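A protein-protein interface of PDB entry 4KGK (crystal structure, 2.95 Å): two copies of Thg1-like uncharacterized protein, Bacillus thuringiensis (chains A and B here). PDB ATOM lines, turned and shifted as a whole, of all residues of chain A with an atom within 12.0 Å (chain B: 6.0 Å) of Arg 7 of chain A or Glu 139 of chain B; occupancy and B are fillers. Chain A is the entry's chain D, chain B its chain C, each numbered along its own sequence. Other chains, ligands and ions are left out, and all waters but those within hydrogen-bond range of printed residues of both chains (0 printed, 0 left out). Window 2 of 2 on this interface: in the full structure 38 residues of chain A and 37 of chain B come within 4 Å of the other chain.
Of chain B, only Glu 139 comes within 4 Å of Arg 7 of chain A. Glu 139 of chain B touches three residues of chain A. Printed residues of chain A within 4 Å of Leu 135 of chain B: Tyr 11 (3.5 Å). Pro 136 of chain B touches one residue of chain A. No residue of chain A comes within 4 Å of Asn 142 of chain B. Printed residues of chain B within 4 Å of Met 8 of chain A: Glu 139 (3.3 Å) and Tyr 143 (3.8 Å). Of the printed residues of chain B, Tyr 11 of chain A touches Leu 135 (3.5 Å), Pro 136 (3.5 Å) and Glu 139 (3.2 Å). Of the printed residues of chain A, Tyr 143 of chain B touches Met 8. The nearest residue of chain B that does not touch Arg 7 of chain A is Asn 142 of chain B (4.5 Å).
No position is printed for both chains.
Hydrophobic or aromatic side chains of chain B that line the printed part of chain A: Leu 135 and Pro 136. Of the 15 printed residues of chain A, 3 touch a printed residue of chain B. Hydrophobic or aromatic side chains of chain A within 4 Å of the printed part of chain B: Met 8 and Tyr 11.
OE1 of Glu 139 of chain B is in hydrogen-bond range of OH of Tyr 11 of chain A (3.2 Å). The guanidinium group (NH1) of Arg 7 of chain A is in salt-bridge range of the side-chain carboxylate (OE2) of Glu 139 of chain B (2.8 Å).
Glu 139 of chain B touches Met 8 of chain A (OE2 to CE, 3.3 Å). CA of Tyr 143 of chain B touches SD of Met 8 of chain A (3.8 Å). CG of Tyr 11 of chain A touches CD2 of Leu 135 of chain B (3.5 Å). Pro 136 of chain B touches Tyr 11 of chain A (CD to CE1, 3.5 Å).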
ATOM      1  N   ASP A   2      27.621   3.583   2.354  1.00  0.00           N
ATOM      2  CA  ASP A   2      26.596   4.020   3.293  1.00  0.00           C
ATOM      3  C   ASP A   2      25.669   2.871   3.676  1.00  0.00           C
ATOM      4  O   ASP A   2      25.934   2.146   4.632  1.00  0.00           O
ATOM      5  CB  ASP A   2      25.786   5.178   2.707  1.00  0.00           C
ATOM      6  N   SER A   3      24.589   2.711   2.918  1.00  0.00           N
ATOM      7  CA  SER A   3      23.594   1.673   3.186  1.00  0.00           C
ATOM      8  C   SER A   3      24.188   0.268   3.133  1.00  0.00           C
ATOM      9  O   SER A   3      23.938  -0.553   4.016  1.00  0.00           O
ATOM     10  CB  SER A   3      22.427   1.786   2.201  1.00  0.00           C
ATOM     11  N   ILE A   4      24.972  -0.005   2.093  1.00  0.00           N
ATOM     12  CA  ILE A   4      25.630  -1.298   1.949  1.00  0.00           C
ATOM     13  C   ILE A   4      26.833  -1.388   2.883  1.00  0.00           C
ATOM     14  O   ILE A   4      27.186  -2.469   3.356  1.00  0.00           O
ATOM     15  CB  ILE A   4      26.095  -1.544   0.502  1.00  0.00           C
ATOM     16  N   GLY A   5      27.457  -0.245   3.144  1.00  0.00           N
ATOM     17  CA  GLY A   5      28.600  -0.185   4.033  1.00  0.00           C
ATOM     18  C   GLY A   5      28.220  -0.438   5.478  1.00  0.00           C
ATOM     19  O   GLY A   5      29.028  -0.929   6.263  1.00  0.00           O
ATOM     20  N   ASP A   6      26.985  -0.099   5.830  1.00  0.00           N
ATOM     21  CA  ASP A   6      26.490  -0.318   7.184  1.00  0.00           C
ATOM     22  C   ASP A   6      26.308  -1.804   7.464  1.00  0.00           C
ATOM     23  O   ASP A   6      26.627  -2.284   8.551  1.00  0.00           O
ATOM     24  CB  ASP A   6      25.171   0.425   7.410  1.00  0.00           C
ATOM     25  CG  ASP A   6      25.357   1.927   7.506  1.00  0.00           C
ATOM     26  OD1 ASP A   6      24.452   2.670   7.066  1.00  0.00           O
ATOM     27  OD2 ASP A   6      26.410   2.368   8.015  1.00  0.00           O
ATOM     28  N   ARG A   7      25.795  -2.529   6.477  1.00  0.00           N
ATOM     29  CA  ARG A   7      25.577  -3.961   6.625  1.00  0.00           C
ATOM     30  C   ARG A   7      26.912  -4.686   6.752  1.00  0.00           C
ATOM     31  O   ARG A   7      27.066  -5.572   7.589  1.00  0.00           O
ATOM     32  CB  ARG A   7      24.788  -4.513   5.435  1.00  0.00           C
ATOM     33  CG  ARG A   7      23.864  -5.671   5.787  1.00  0.00           C
ATOM     34  CD  ARG A   7      23.199  -6.264   4.552  1.00  0.00           C
ATOM     35  NE  ARG A   7      23.066  -5.294   3.470  1.00  0.00           N
ATOM     36  CZ  ARG A   7      23.668  -5.406   2.289  1.00  0.00           C
ATOM     37  NH1 ARG A   7      24.438  -6.456   2.032  1.00  0.00           N
ATOM     38  NH2 ARG A   7      23.494  -4.475   1.362  1.00  0.00           N
ATOM     39  N   MET A   8      27.874  -4.292   5.922  1.00  0.00           N
ATOM     40  CA  MET A   8      29.195  -4.918   5.916  1.00  0.00           C
ATOM     41  C   MET A   8      29.950  -4.669   7.214  1.00  0.00           C
ATOM     42  O   MET A   8      30.666  -5.545   7.698  1.00  0.00           O
ATOM     43  CB  MET A   8      30.024  -4.419   4.730  1.00  0.00           C
ATOM     44  CG  MET A   8      29.501  -4.842   3.365  1.00  0.00           C
ATOM     45  SD  MET A   8      29.545  -6.626   3.105  1.00  0.00           S
ATOM     46  CE  MET A   8      27.840  -7.074   3.436  1.00  0.00           C
ATOM     47  N   LYS A   9      29.791  -3.472   7.769  1.00  0.00           N
ATOM     48  CA  LYS A   9      30.464  -3.110   9.012  1.00  0.00           C
ATOM     49  C   LYS A   9      30.005  -3.965  10.189  1.00  0.00           C
ATOM     50  O   LYS A   9      30.803  -4.302  11.060  1.00  0.00           O
ATOM     51  CB  LYS A   9      30.272  -1.624   9.324  1.00  0.00           C
ATOM     52  CG  LYS A   9      31.310  -0.718   8.678  1.00  0.00           C
ATOM     53  CD  LYS A   9      32.712  -1.076   9.152  1.00  0.00           C
ATOM     54  CE  LYS A   9      33.767  -0.187   8.510  1.00  0.00           C
ATOM     55  NZ  LYS A   9      35.144  -0.577   8.922  1.00  0.00           N
ATOM     56  N   ARG A  10      28.723  -4.318  10.209  1.00  0.00           N
ATOM     57  CA  ARG A  10      28.186  -5.163  11.269  1.00  0.00           C
ATOM     58  C   ARG A  10      28.844  -6.541  11.300  1.00  0.00           C
ATOM     59  O   ARG A  10      29.103  -7.084  12.377  1.00  0.00           O
ATOM     60  CB  ARG A  10      26.666  -5.299  11.148  1.00  0.00           C
ATOM     61  CG  ARG A  10      25.893  -4.170  11.807  1.00  0.00           C
ATOM     62  CD  ARG A  10      24.399  -4.467  11.869  1.00  0.00           C
ATOM     63  NE  ARG A  10      23.691  -4.013  10.677  1.00  0.00           N
ATOM     64  CZ  ARG A  10      23.406  -4.785   9.635  1.00  0.00           C
ATOM     65  NH1 ARG A  10      23.768  -6.060   9.631  1.00  0.00           N
ATOM     66  NH2 ARG A  10      22.756  -4.280   8.594  1.00  0.00           N
ATOM     67  N   TYR A  11      29.111  -7.101  10.123  1.00  0.00           N
ATOM     68  CA  TYR A  11      29.810  -8.379  10.023  1.00  0.00           C
ATOM     69  C   TYR A  11      31.228  -8.243  10.560  1.00  0.00           C
ATOM     70  O   TYR A  11      31.727  -9.117  11.269  1.00  0.00           O
ATOM     71  CB  TYR A  11      29.859  -8.865   8.574  1.00  0.00           C
ATOM     72  CG  TYR A  11      28.518  -9.273   8.011  1.00  0.00           C
ATOM     73  CD1 TYR A  11      27.931 -10.476   8.373  1.00  0.00           C
ATOM     74  CD2 TYR A  11      27.845  -8.462   7.108  1.00  0.00           C
ATOM     75  CE1 TYR A  11      26.706 -10.855   7.863  1.00  0.00           C
ATOM     76  CE2 TYR A  11      26.620  -8.831   6.589  1.00  0.00           C
ATOM     77  CZ  TYR A  11      26.054 -10.030   6.970  1.00  0.00           C
ATOM     78  OH  TYR A  11      24.833 -10.407   6.461  1.00  0.00           O
ATOM     79  N   GLU A  12      31.871  -7.135  10.207  1.00  0.00           N
ATOM     80  CA  GLU A  12      33.228  -6.848  10.648  1.00  0.00           C
ATOM     81  C   GLU A  12      33.266  -6.589  12.153  1.00  0.00           C
ATOM     82  O   GLU A  12      34.155  -7.074  12.854  1.00  0.00           O
ATOM     83  CB  GLU A  12      33.780  -5.639   9.893  1.00  0.00           C
ATOM     84  CG  GLU A  12      35.199  -5.259  10.271  1.00  0.00           C
ATOM     85  CD  GLU A  12      35.616  -3.921   9.693  1.00  0.00           C
ATOM     86  OE1 GLU A  12      34.948  -3.445   8.749  1.00  0.00           O
ATOM     87  OE2 GLU A  12      36.608  -3.343  10.187  1.00  0.00           O
ATOM     88  N   ASN A  13      32.294  -5.827  12.644  1.00  0.00           N
ATOM     89  CA  ASN A  13      32.217  -5.502  14.063  1.00  0.00           C
ATOM     90  C   ASN A  13      31.837  -6.696  14.927  1.00  0.00           C
ATOM     91  O   ASN A  13      31.983  -6.657  16.146  1.00  0.00           O
ATOM     92  CB  ASN A  13      31.239  -4.355  14.305  1.00  0.00           C
ATOM     93  CG  ASN A  13      31.688  -3.065  13.658  1.00  0.00           C
ATOM     94  OD1 ASN A  13      32.883  -2.835  13.472  1.00  0.00           O
ATOM     95  ND2 ASN A  13      30.730  -2.213  13.310  1.00  0.00           N
ATOM     96  N   ALA A  14      31.345  -7.755  14.291  1.00  0.00           N
ATOM     97  CA  ALA A  14      31.009  -8.985  15.002  1.00  0.00           C
ATOM     98  C   ALA A  14      32.257  -9.591  15.630  1.00  0.00           C
ATOM     99  O   ALA A  14      32.178 -10.325  16.614  1.00  0.00           O
ATOM    100  CB  ALA A  14      30.352  -9.980  14.063  1.00  0.00           C
ATOM    101  N   TYR A  15      33.412  -9.281  15.052  1.00  0.00           N
ATOM    102  CA  TYR A  15      34.678  -9.744  15.601  1.00  0.00           C
ATOM    103  C   TYR A  15      35.612  -8.583  15.911  1.00  0.00           C
ATOM    104  O   TYR A  15      36.834  -8.707  15.840  1.00  0.00           O
ATOM    105  CB  TYR A  15      35.324 -10.783  14.683  1.00  0.00           C
ATOM    106  CG  TYR A  15      34.631 -12.119  14.785  1.00  0.00           C
ATOM    107  CD1 TYR A  15      35.067 -13.078  15.688  1.00  0.00           C
ATOM    108  CD2 TYR A  15      33.517 -12.406  14.006  1.00  0.00           C
ATOM    109  CE1 TYR A  15      34.427 -14.295  15.800  1.00  0.00           C
ATOM    110  CE2 TYR A  15      32.872 -13.621  14.108  1.00  0.00           C
ATOM    111  CZ  TYR A  15      33.330 -14.561  15.007  1.00  0.00           C
ATOM    112  OH  TYR A  15      32.692 -15.773  15.117  1.00  0.00           O
ATOM    113  N   ARG A  16      35.010  -7.452  16.261  1.00  0.00           N
ATOM    114  CA  ARG A  16      35.750  -6.316  16.780  1.00  0.00           C
ATOM    115  C   ARG A  16      35.780  -6.427  18.300  1.00  0.00           C
ATOM    116  O   ARG A  16      34.931  -5.865  18.993  1.00  0.00           O
ATOM    117  CB  ARG A  16      35.089  -5.008  16.348  1.00  0.00           C
ATOM    118  CG  ARG A  16      35.816  -3.754  16.802  1.00  0.00           C
ATOM    119  CD  ARG A  16      35.095  -2.502  16.327  1.00  0.00           C
ATOM    120  NE  ARG A  16      35.720  -1.286  16.842  1.00  0.00           N
ATOM    121  CZ  ARG A  16      36.754  -0.678  16.269  1.00  0.00           C
ATOM    122  NH1 ARG A  16      37.287  -1.172  15.159  1.00  0.00           N
ATOM    123  NH2 ARG A  16      37.258   0.424  16.807  1.00  0.00           N
ATOM    124  N   LEU B 135      31.792 -14.136   6.545  1.00  0.00           N
ATOM    125  CA  LEU B 135      30.695 -13.621   5.739  1.00  0.00           C
ATOM    126  C   LEU B 135      29.853 -14.764   5.195  1.00  0.00           C
ATOM    127  O   LEU B 135      30.393 -15.751   4.702  1.00  0.00           O
ATOM    128  CB  LEU B 135      31.228 -12.799   4.564  1.00  0.00           C
ATOM    129  CG  LEU B 135      31.677 -11.363   4.822  1.00  0.00           C
ATOM    130  CD1 LEU B 135      32.129 -10.719   3.523  1.00  0.00           C
ATOM    131  CD2 LEU B 135      30.553 -10.563   5.450  1.00  0.00           C
ATOM    132  N   PRO B 136      28.523 -14.634   5.285  1.00  0.00           N
ATOM    133  CA  PRO B 136      27.620 -15.587   4.631  1.00  0.00           C
ATOM    134  C   PRO B 136      27.826 -15.560   3.118  1.00  0.00           C
ATOM    135  O   PRO B 136      28.145 -14.503   2.571  1.00  0.00           O
ATOM    136  CB  PRO B 136      26.227 -15.065   5.002  1.00  0.00           C
ATOM    137  CG  PRO B 136      26.436 -13.639   5.407  1.00  0.00           C
ATOM    138  CD  PRO B 136      27.793 -13.594   6.026  1.00  0.00           C
ATOM    139  N   GLN B 137      27.650 -16.706   2.464  1.00  0.00           N
ATOM    140  CA  GLN B 137      27.961 -16.863   1.042  1.00  0.00           C
ATOM    141  C   GLN B 137      27.351 -15.787   0.146  1.00  0.00           C
ATOM    142  O   GLN B 137      28.015 -15.264  -0.748  1.00  0.00           O
ATOM    143  CB  GLN B 137      27.534 -18.249   0.552  1.00  0.00           C
ATOM    144  CG  GLN B 137      28.376 -19.389   1.103  1.00  0.00           C
ATOM    145  CD  GLN B 137      27.903 -20.748   0.625  1.00  0.00           C
ATOM    146  OE1 GLN B 137      26.738 -21.113   0.801  1.00  0.00           O
ATOM    147  NE2 GLN B 137      28.804 -21.504   0.010  1.00  0.00           N
ATOM    148  N   ASP B 138      26.088 -15.456   0.395  1.00  0.00           N
ATOM    149  CA  ASP B 138      25.386 -14.461  -0.410  1.00  0.00           C
ATOM    150  C   ASP B 138      25.865 -13.032  -0.148  1.00  0.00           C
ATOM    151  O   ASP B 138      25.424 -12.095  -0.810  1.00  0.00           O
ATOM    152  CB  ASP B 138      23.871 -14.571  -0.203  1.00  0.00           C
ATOM    153  CG  ASP B 138      23.499 -14.914   1.228  1.00  0.00           C
ATOM    154  OD1 ASP B 138      22.562 -14.288   1.771  1.00  0.00           O
ATOM    155  OD2 ASP B 138      24.139 -15.817   1.808  1.00  0.00           O
ATOM    156  N   GLU B 139      26.771 -12.869   0.810  1.00  0.00           N
ATOM    157  CA  GLU B 139      27.296 -11.548   1.142  1.00  0.00           C
ATOM    158  C   GLU B 139      28.767 -11.376   0.767  1.00  0.00           C
ATOM    159  O   GLU B 139      29.376 -10.354   1.086  1.00  0.00           O
ATOM    160  CB  GLU B 139      27.102 -11.248   2.632  1.00  0.00           C
ATOM    161  CG  GLU B 139      25.657 -11.009   3.049  1.00  0.00           C
ATOM    162  CD  GLU B 139      25.193  -9.581   2.808  1.00  0.00           C
ATOM    163  OE1 GLU B 139      24.374  -9.085   3.608  1.00  0.00           O
ATOM    164  OE2 GLU B 139      25.639  -8.953   1.822  1.00  0.00           O
ATOM    165  N   VAL B 140      29.337 -12.371   0.095  1.00  0.00           N
ATOM    166  CA  VAL B 140      30.750 -12.314  -0.269  1.00  0.00           C
ATOM    167  C   VAL B 140      30.986 -11.360  -1.435  1.00  0.00           C
ATOM    168  O   VAL B 140      31.912 -10.550  -1.409  1.00  0.00           O
ATOM    169  CB  VAL B 140      31.315 -13.705  -0.622  1.00  0.00           C
ATOM    170  CG1 VAL B 140      32.817 -13.618  -0.854  1.00  0.00           C
ATOM    171  CG2 VAL B 140      31.005 -14.706   0.483  1.00  0.00           C
ATOM    172  N   ALA B 141      30.142 -11.460  -2.456  1.00  0.00           N
ATOM    173  CA  ALA B 141      30.265 -10.604  -3.630  1.00  0.00           C
ATOM    174  C   ALA B 141      29.983  -9.150  -3.276  1.00  0.00           C
ATOM    175  O   ALA B 141      30.610  -8.239  -3.813  1.00  0.00           O
ATOM    176  CB  ALA B 141      29.332 -11.076  -4.730  1.00  0.00           C
ATOM    177  N   ASN B 142      29.040  -8.938  -2.362  1.00  0.00           N
ATOM    178  CA  ASN B 142      28.679  -7.591  -1.934  1.00  0.00           C
ATOM    179  C   ASN B 142      29.819  -6.875  -1.215  1.00  0.00           C
ATOM    180  O   ASN B 142      29.896  -5.646  -1.230  1.00  0.00           O
ATOM    181  CB  ASN B 142      27.432  -7.622  -1.047  1.00  0.00           C
ATOM    182  CG  ASN B 142      26.216  -8.157  -1.774  1.00  0.00           C
ATOM    183  OD1 ASN B 142      25.450  -7.399  -2.369  1.00  0.00           O
ATOM    184  ND2 ASN B 142      26.033  -9.472  -1.736  1.00  0.00           N
ATOM    185  N   TYR B 143      30.702  -7.649  -0.590  1.00  0.00           N
ATOM    186  CA  TYR B 143      31.863  -7.092   0.096  1.00  0.00           C
ATOM    187  C   TYR B 143      32.827  -6.440  -0.888  1.00  0.00           C
ATOM    188  O   TYR B 143      33.201  -5.278  -0.726  1.00  0.00           O
ATOM    189  CB  TYR B 143      32.590  -8.175   0.898  1.00  0.00           C
ATOM    190  CG  TYR B 143      33.957  -7.753   1.394  1.00  0.00           C
ATOM    191  CD1 TYR B 143      34.090  -6.954   2.522  1.00  0.00           C
ATOM    192  CD2 TYR B 143      35.114  -8.156   0.735  1.00  0.00           C
ATOM    193  CE1 TYR B 143      35.337  -6.564   2.977  1.00  0.00           C
ATOM    194  CE2 TYR B 143      36.364  -7.771   1.184  1.00  0.00           C
ATOM    195  CZ  TYR B 143      36.470  -6.978   2.306  1.00  0.00           C
ATOM    196  OH  TYR B 143      37.712  -6.593   2.757  1.00  0.00           O
ATOM    197  N   PHE B 144      33.227  -7.195  -1.906  1.00  0.00           N
ATOM    198  CA  PHE B 144      34.163  -6.693  -2.909  1.00  0.00           C
ATOM    199  C   PHE B 144      33.553  -5.578  -3.757  1.00  0.00           C
ATOM    200  O   PHE B 144      34.266  -4.695  -4.231  1.00  0.00           O
ATOM    201  CB  PHE B 144      34.671  -7.831  -3.796  1.00  0.00           C
ATOM    202  CG  PHE B 144      35.553  -8.809  -3.076  1.00  0.00           C
ATOM    203  CD1 PHE B 144      36.897  -8.530  -2.876  1.00  0.00           C
ATOM    204  CD2 PHE B 144      35.044 -10.004  -2.596  1.00  0.00           C
ATOM    205  CE1 PHE B 144      37.716  -9.424  -2.214  1.00  0.00           C
ATOM    206  CE2 PHE B 144      35.859 -10.904  -1.932  1.00  0.00           C
ATOM    207  CZ  PHE B 144      37.197 -10.613  -1.742  1.00  0.00           C
ATOM    208  N   TYR B 238      30.718 -20.435  -4.032  1.00  0.00           N
ATOM    209  CA  TYR B 238      29.906 -21.640  -4.148  1.00  0.00           C
ATOM    210  C   TYR B 238      30.676 -22.717  -4.902  1.00  0.00           C
ATOM    211  O   TYR B 238      30.843 -22.633  -6.116  1.00  0.00           O
ATOM    212  CB  TYR B 238      28.589 -21.332  -4.864  1.00  0.00           C
ATOM    213  CG  TYR B 238      27.756 -20.261  -4.190  1.00  0.00           C
ATOM    214  CD1 TYR B 238      26.838 -20.588  -3.197  1.00  0.00           C
ATOM    215  CD2 TYR B 238      27.885 -18.924  -4.548  1.00  0.00           C
ATOM    216  CE1 TYR B 238      26.076 -19.612  -2.579  1.00  0.00           C
ATOM    217  CE2 TYR B 238      27.125 -17.942  -3.936  1.00  0.00           C
ATOM    218  CZ  TYR B 238      26.223 -18.292  -2.953  1.00  0.00           C
ATOM    219  OH  TYR B 238      25.467 -17.318  -2.342  1.00  0.00           O
